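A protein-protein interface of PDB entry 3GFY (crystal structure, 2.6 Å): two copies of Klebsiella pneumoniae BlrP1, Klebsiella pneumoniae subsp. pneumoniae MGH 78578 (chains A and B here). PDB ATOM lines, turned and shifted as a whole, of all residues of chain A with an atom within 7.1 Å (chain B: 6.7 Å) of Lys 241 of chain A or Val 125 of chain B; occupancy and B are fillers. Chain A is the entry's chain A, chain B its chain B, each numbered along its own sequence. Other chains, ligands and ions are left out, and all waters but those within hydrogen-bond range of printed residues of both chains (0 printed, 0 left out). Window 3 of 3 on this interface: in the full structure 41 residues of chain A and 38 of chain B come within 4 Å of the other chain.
Of the 7 printed residues of chain B, 5 touch a printed residue of chain A.
Among the printed residues, 8 pairs touch across the chains.
Among the printed residues, no Asp or Glu carboxylate lies within 4 Å of a Lys or Arg side-chain nitrogen of the other chain.
No position is printed for both chains.
Of the 8 pairs that touch across the chains among the printed residues, none has its exchanged pair printed and touching as well.
The backbone NH of Val 125 of chain B sits at hydrogen-bond distance from the side-chain carboxylate of Asp 275 of chain A (3.0 Å).
O of Ser 193 of chain A is in hydrogen-bond range of N of Gln 243 of chain A, 3.5 Å away.
NE2 of Gln 276 of chain A is in hydrogen-bond range of O of Gly 240 of chain A, 2.8 Å away.
The side-chain amide nitrogen of Gln 276 of chain A sits close to the backbone carbonyl oxygen of His 242 of chain A (3.2 Å).
N of Arg 273 of chain A is in hydrogen-bond range of OE1 of Gln 276 of chain A (3.3 Å).
The side-chain hydroxyl (OH) of Tyr 92 of chain B lies within hydrogen-bond range of the backbone NH (N) of Gly 124 of chain B.
OG1 of Thr 126 of chain B lies within hydrogen-bond range of ND2 of Asn 130 of chain B.
Among the printed residues, merely in contact across the chains: Asp 275 of chain A with Gly 124 of chain B, Arg 191 of chain A with Glu 127 of chain B, Gln 243 of chain A with Asn 130 of chain B, Lys 241 of chain A with Val 125 of chain B, Lys 241 of chain A with Thr 126 of chain B, Arg 273 of chain A with Val 125 of chain B and Gln 276 of chain A with Thr 126 of chain B.
Of the printed residues of chain B, Arg 191 of chain A touches Glu 127 (3.4 Å).
Lys 241 of chain A touches just these residues of chain B: Val 125 and Thr 126.
Of the printed residues of chain B, Asp 275 of chain A touches Gly 124 and Val 125.
Val 125 of chain B touches three residues of chain A.
Of the printed residues of chain A, Thr 126 of chain B touches Lys 241 (3.7 Å) and Gln 276 (3.95 Å).
Of the printed residues of chain A, Glu 127 of chain B touches Arg 191 (3.4 Å).
The nearest printed residue of chain B that does not touch Arg 273 of chain A is Gly 124 of chain B (6.8 Å).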
ATOM      1  N   ARG A 191     -36.183   8.931 -20.498  1.00  0.00           N
ATOM      2  CA  ARG A 191     -35.247   8.329 -19.563  1.00  0.00           C
ATOM      3  C   ARG A 191     -34.912   6.904 -19.993  1.00  0.00           C
ATOM      4  O   ARG A 191     -35.790   6.157 -20.425  1.00  0.00           O
ATOM      5  CB  ARG A 191     -35.875   8.324 -18.162  1.00  0.00           C
ATOM      6  CG  ARG A 191     -34.995   7.773 -17.048  1.00  0.00           C
ATOM      7  CD  ARG A 191     -35.708   7.808 -15.696  1.00  0.00           C
ATOM      8  NE  ARG A 191     -36.632   6.686 -15.508  1.00  0.00           N
ATOM      9  CZ  ARG A 191     -36.283   5.487 -15.039  1.00  0.00           C
ATOM     10  NH1 ARG A 191     -35.019   5.233 -14.710  1.00  0.00           N
ATOM     11  NH2 ARG A 191     -37.199   4.533 -14.902  1.00  0.00           N
ATOM     12  N   VAL A 192     -33.637   6.541 -19.882  1.00  0.00           N
ATOM     13  CA  VAL A 192     -33.214   5.157 -20.056  1.00  0.00           C
ATOM     14  C   VAL A 192     -33.428   4.411 -18.744  1.00  0.00           C
ATOM     15  O   VAL A 192     -32.861   4.782 -17.715  1.00  0.00           O
ATOM     16  CB  VAL A 192     -31.726   5.057 -20.452  1.00  0.00           C
ATOM     17  CG1 VAL A 192     -31.349   3.609 -20.738  1.00  0.00           C
ATOM     18  CG2 VAL A 192     -31.432   5.933 -21.653  1.00  0.00           C
ATOM     19  N   SER A 193     -34.247   3.365 -18.781  1.00  0.00           N
ATOM     20  CA  SER A 193     -34.521   2.559 -17.595  1.00  0.00           C
ATOM     21  C   SER A 193     -33.373   1.599 -17.306  1.00  0.00           C
ATOM     22  O   SER A 193     -32.838   1.560 -16.194  1.00  0.00           O
ATOM     23  CB  SER A 193     -35.822   1.775 -17.770  1.00  0.00           C
ATOM     24  OG  SER A 193     -36.000   0.840 -16.719  1.00  0.00           O
ATOM     25  N   PRO A 238     -19.879   4.753 -17.237  1.00  0.00           N
ATOM     26  CA  PRO A 238     -20.327   3.976 -16.074  1.00  0.00           C
ATOM     27  C   PRO A 238     -21.837   3.754 -16.114  1.00  0.00           C
ATOM     28  O   PRO A 238     -22.552   4.485 -16.806  1.00  0.00           O
ATOM     29  CB  PRO A 238     -19.946   4.868 -14.890  1.00  0.00           C
ATOM     30  CG  PRO A 238     -20.019   6.254 -15.426  1.00  0.00           C
ATOM     31  CD  PRO A 238     -19.736   6.185 -16.909  1.00  0.00           C
ATOM     32  N   LEU A 239     -22.311   2.744 -15.392  1.00  0.00           N
ATOM     33  CA  LEU A 239     -23.729   2.400 -15.415  1.00  0.00           C
ATOM     34  C   LEU A 239     -24.565   3.411 -14.632  1.00  0.00           C
ATOM     35  O   LEU A 239     -25.646   3.802 -15.072  1.00  0.00           O
ATOM     36  CB  LEU A 239     -23.951   0.981 -14.884  1.00  0.00           C
ATOM     37  CG  LEU A 239     -25.298   0.330 -15.207  1.00  0.00           C
ATOM     38  CD1 LEU A 239     -25.599   0.366 -16.704  1.00  0.00           C
ATOM     39  CD2 LEU A 239     -25.343  -1.098 -14.680  1.00  0.00           C
ATOM     40  N   GLY A 240     -24.051   3.832 -13.479  1.00  0.00           N
ATOM     41  CA  GLY A 240     -24.708   4.850 -12.664  1.00  0.00           C
ATOM     42  C   GLY A 240     -25.914   4.327 -11.911  1.00  0.00           C
ATOM     43  O   GLY A 240     -25.791   3.440 -11.063  1.00  0.00           O
ATOM     44  N   LYS A 241     -27.081   4.880 -12.230  1.00  0.00           N
ATOM     45  CA  LYS A 241     -28.324   4.535 -11.542  1.00  0.00           C
ATOM     46  C   LYS A 241     -29.256   3.705 -12.434  1.00  0.00           C
ATOM     47  O   LYS A 241     -30.480   3.716 -12.257  1.00  0.00           O
ATOM     48  CB  LYS A 241     -29.033   5.813 -11.066  1.00  0.00           C
ATOM     49  CG  LYS A 241     -28.196   6.696 -10.133  1.00  0.00           C
ATOM     50  CD  LYS A 241     -28.862   8.048  -9.883  1.00  0.00           C
ATOM     51  CE  LYS A 241     -28.129   8.869  -8.817  1.00  0.00           C
ATOM     52  NZ  LYS A 241     -26.752   9.292  -9.220  1.00  0.00           N
ATOM     53  N   HIS A 242     -28.667   2.981 -13.385  1.00  0.00           N
ATOM     54  CA  HIS A 242     -29.428   2.209 -14.368  1.00  0.00           C
ATOM     55  C   HIS A 242     -29.246   0.708 -14.170  1.00  0.00           C
ATOM     56  O   HIS A 242     -28.225   0.274 -13.655  1.00  0.00           O
ATOM     57  CB  HIS A 242     -29.002   2.595 -15.789  1.00  0.00           C
ATOM     58  CG  HIS A 242     -29.071   4.065 -16.063  1.00  0.00           C
ATOM     59  ND1 HIS A 242     -27.946   4.847 -16.213  1.00  0.00           N
ATOM     60  CD2 HIS A 242     -30.129   4.897 -16.207  1.00  0.00           C
ATOM     61  CE1 HIS A 242     -28.308   6.097 -16.440  1.00  0.00           C
ATOM     62  NE2 HIS A 242     -29.628   6.154 -16.441  1.00  0.00           N
ATOM     63  N   GLN A 243     -30.238  -0.078 -14.585  1.00  0.00           N
ATOM     64  CA  GLN A 243     -30.179  -1.538 -14.470  1.00  0.00           C
ATOM     65  C   GLN A 243     -29.438  -2.198 -15.632  1.00  0.00           C
ATOM     66  O   GLN A 243     -29.030  -1.525 -16.577  1.00  0.00           O
ATOM     67  CB  GLN A 243     -31.583  -2.137 -14.367  1.00  0.00           C
ATOM     68  CG  GLN A 243     -32.207  -2.097 -12.990  1.00  0.00           C
ATOM     69  CD  GLN A 243     -33.400  -3.034 -12.869  1.00  0.00           C
ATOM     70  OE1 GLN A 243     -33.853  -3.618 -13.856  1.00  0.00           O
ATOM     71  NE2 GLN A 243     -33.912  -3.182 -11.655  1.00  0.00           N
ATOM     72  N   LEU A 272     -20.253  -2.847  -9.598  1.00  0.00           N
ATOM     73  CA  LEU A 272     -21.707  -2.799  -9.684  1.00  0.00           C
ATOM     74  C   LEU A 272     -22.331  -3.258  -8.374  1.00  0.00           C
ATOM     75  O   LEU A 272     -21.659  -3.850  -7.530  1.00  0.00           O
ATOM     76  CB  LEU A 272     -22.210  -3.669 -10.840  1.00  0.00           C
ATOM     77  CG  LEU A 272     -21.665  -3.401 -12.245  1.00  0.00           C
ATOM     78  CD1 LEU A 272     -22.096  -4.512 -13.189  1.00  0.00           C
ATOM     79  CD2 LEU A 272     -22.109  -2.039 -12.767  1.00  0.00           C
ATOM     80  N   ARG A 273     -23.617  -2.968  -8.207  1.00  0.00           N
ATOM     81  CA  ARG A 273     -24.375  -3.439  -7.056  1.00  0.00           C
ATOM     82  C   ARG A 273     -25.316  -4.574  -7.473  1.00  0.00           C
ATOM     83  O   ARG A 273     -25.707  -4.652  -8.640  1.00  0.00           O
ATOM     84  CB  ARG A 273     -25.145  -2.280  -6.413  1.00  0.00           C
ATOM     85  CG  ARG A 273     -24.250  -1.245  -5.715  1.00  0.00           C
ATOM     86  CD  ARG A 273     -23.354  -1.882  -4.655  1.00  0.00           C
ATOM     87  NE  ARG A 273     -24.121  -2.469  -3.558  1.00  0.00           N
ATOM     88  CZ  ARG A 273     -23.625  -3.319  -2.662  1.00  0.00           C
ATOM     89  NH1 ARG A 273     -22.352  -3.696  -2.727  1.00  0.00           N
ATOM     90  NH2 ARG A 273     -24.405  -3.801  -1.699  1.00  0.00           N
ATOM     91  N   PRO A 274     -25.643  -5.483  -6.533  1.00  0.00           N
ATOM     92  CA  PRO A 274     -26.560  -6.593  -6.801  1.00  0.00           C
ATOM     93  C   PRO A 274     -27.923  -6.150  -7.343  1.00  0.00           C
ATOM     94  O   PRO A 274     -28.399  -6.702  -8.338  1.00  0.00           O
ATOM     95  CB  PRO A 274     -26.727  -7.237  -5.423  1.00  0.00           C
ATOM     96  CG  PRO A 274     -25.469  -6.915  -4.708  1.00  0.00           C
ATOM     97  CD  PRO A 274     -25.124  -5.532  -5.154  1.00  0.00           C
ATOM     98  N   ASP A 275     -28.523  -5.147  -6.702  1.00  0.00           N
ATOM     99  CA  ASP A 275     -29.844  -4.622  -7.082  1.00  0.00           C
ATOM    100  C   ASP A 275     -29.853  -3.909  -8.435  1.00  0.00           C
ATOM    101  O   ASP A 275     -30.904  -3.511  -8.934  1.00  0.00           O
ATOM    102  CB  ASP A 275     -30.370  -3.681  -5.995  1.00  0.00           C
ATOM    103  CG  ASP A 275     -29.285  -2.784  -5.428  1.00  0.00           C
ATOM    104  OD1 ASP A 275     -28.415  -3.290  -4.685  1.00  0.00           O
ATOM    105  OD2 ASP A 275     -29.304  -1.572  -5.722  1.00  0.00           O
ATOM    106  N   GLN A 276     -28.670  -3.764  -9.018  1.00  0.00           N
ATOM    107  CA  GLN A 276     -28.490  -3.115 -10.301  1.00  0.00           C
ATOM    108  C   GLN A 276     -28.517  -4.142 -11.433  1.00  0.00           C
ATOM    109  O   GLN A 276     -28.701  -3.791 -12.602  1.00  0.00           O
ATOM    110  CB  GLN A 276     -27.150  -2.387 -10.292  1.00  0.00           C
ATOM    111  CG  GLN A 276     -27.029  -1.271 -11.280  1.00  0.00           C
ATOM    112  CD  GLN A 276     -25.815  -0.411 -11.033  1.00  0.00           C
ATOM    113  OE1 GLN A 276     -24.926  -0.770 -10.259  1.00  0.00           O
ATOM    114  NE2 GLN A 276     -25.769   0.738 -11.693  1.00  0.00           N
ATOM    115  N   TYR B  92     -31.639  -6.667   1.641  1.00  0.00           N
ATOM    116  CA  TYR B  92     -31.429  -5.475   2.450  1.00  0.00           C
ATOM    117  C   TYR B  92     -32.764  -4.933   2.948  1.00  0.00           C
ATOM    118  O   TYR B  92     -33.807  -5.189   2.348  1.00  0.00           O
ATOM    119  CB  TYR B  92     -30.656  -4.409   1.655  1.00  0.00           C
ATOM    120  CG  TYR B  92     -31.388  -3.848   0.450  1.00  0.00           C
ATOM    121  CD1 TYR B  92     -31.418  -4.540  -0.765  1.00  0.00           C
ATOM    122  CD2 TYR B  92     -32.036  -2.615   0.519  1.00  0.00           C
ATOM    123  CE1 TYR B  92     -32.089  -4.026  -1.870  1.00  0.00           C
ATOM    124  CE2 TYR B  92     -32.706  -2.092  -0.582  1.00  0.00           C
ATOM    125  CZ  TYR B  92     -32.731  -2.801  -1.771  1.00  0.00           C
ATOM    126  OH  TYR B  92     -33.392  -2.279  -2.859  1.00  0.00           O
ATOM    127  N   PHE B 123     -34.055   2.392  -1.523  1.00  0.00           N
ATOM    128  CA  PHE B 123     -34.450   1.370  -2.485  1.00  0.00           C
ATOM    129  C   PHE B 123     -33.312   1.041  -3.447  1.00  0.00           C
ATOM    130  O   PHE B 123     -33.517   0.947  -4.660  1.00  0.00           O
ATOM    131  CB  PHE B 123     -35.697   1.809  -3.254  1.00  0.00           C
ATOM    132  CG  PHE B 123     -36.937   1.879  -2.413  1.00  0.00           C
ATOM    133  CD1 PHE B 123     -37.725   0.753  -2.221  1.00  0.00           C
ATOM    134  CD2 PHE B 123     -37.327   3.076  -1.824  1.00  0.00           C
ATOM    135  CE1 PHE B 123     -38.879   0.815  -1.441  1.00  0.00           C
ATOM    136  CE2 PHE B 123     -38.479   3.147  -1.045  1.00  0.00           C
ATOM    137  CZ  PHE B 123     -39.254   2.016  -0.855  1.00  0.00           C
ATOM    138  N   GLY B 124     -32.114   0.868  -2.897  1.00  0.00           N
ATOM    139  CA  GLY B 124     -30.941   0.516  -3.690  1.00  0.00           C
ATOM    140  C   GLY B 124     -30.361   1.686  -4.457  1.00  0.00           C
ATOM    141  O   GLY B 124     -30.761   2.834  -4.252  1.00  0.00           O
ATOM    142  N   VAL B 125     -29.416   1.391  -5.349  1.00  0.00           N
ATOM    143  CA  VAL B 125     -28.751   2.425  -6.142  1.00  0.00           C
ATOM    144  C   VAL B 125     -29.563   2.889  -7.353  1.00  0.00           C
ATOM    145  O   VAL B 125     -29.292   3.952  -7.913  1.00  0.00           O
ATOM    146  CB  VAL B 125     -27.339   1.987  -6.618  1.00  0.00           C
ATOM    147  CG1 VAL B 125     -26.382   1.882  -5.439  1.00  0.00           C
ATOM    148  CG2 VAL B 125     -27.399   0.678  -7.404  1.00  0.00           C
ATOM    149  N   THR B 126     -30.546   2.093  -7.763  1.00  0.00           N
ATOM    150  CA  THR B 126     -31.368   2.449  -8.915  1.00  0.00           C
ATOM    151  C   THR B 126     -32.662   3.121  -8.466  1.00  0.00           C
ATOM    152  O   THR B 126     -32.928   3.224  -7.264  1.00  0.00           O
ATOM    153  CB  THR B 126     -31.679   1.229  -9.818  1.00  0.00           C
ATOM    154  OG1 THR B 126     -32.615   0.362  -9.166  1.00  0.00           O
ATOM    155  CG2 THR B 126     -30.399   0.455 -10.143  1.00  0.00           C
ATOM    156  N   GLU B 127     -33.450   3.581  -9.436  1.00  0.00           N
ATOM    157  CA  GLU B 127     -34.721   4.256  -9.167  1.00  0.00           C
ATOM    158  C   GLU B 127     -35.635   3.372  -8.327  1.00  0.00           C
ATOM    159  O   GLU B 127     -35.751   2.178  -8.599  1.00  0.00           O
ATOM    160  CB  GLU B 127     -35.422   4.628 -10.478  1.00  0.00           C
ATOM    161  CG  GLU B 127     -34.685   5.663 -11.324  1.00  0.00           C
ATOM    162  CD  GLU B 127     -34.866   7.084 -10.822  1.00  0.00           C
ATOM    163  OE1 GLU B 127     -35.956   7.406 -10.298  1.00  0.00           O
ATOM    164  OE2 GLU B 127     -33.917   7.884 -10.960  1.00  0.00           O
ATOM    165  N   ASN B 130     -37.930   0.592  -9.559  1.00  0.00           N
ATOM    166  CA  ASN B 130     -37.427  -0.743  -9.903  1.00  0.00           C
ATOM    167  C   ASN B 130     -37.617  -1.773  -8.786  1.00  0.00           C
ATOM    168  O   ASN B 130     -37.338  -2.959  -8.972  1.00  0.00           O
ATOM    169  CB  ASN B 130     -35.954  -0.684 -10.318  1.00  0.00           C
ATOM    170  CG  ASN B 130     -35.742   0.064 -11.623  1.00  0.00           C
ATOM    171  OD1 ASN B 130     -36.526  -0.063 -12.563  1.00  0.00           O
ATOM    172  ND2 ASN B 130     -34.673   0.847 -11.685  1.00  0.00           N
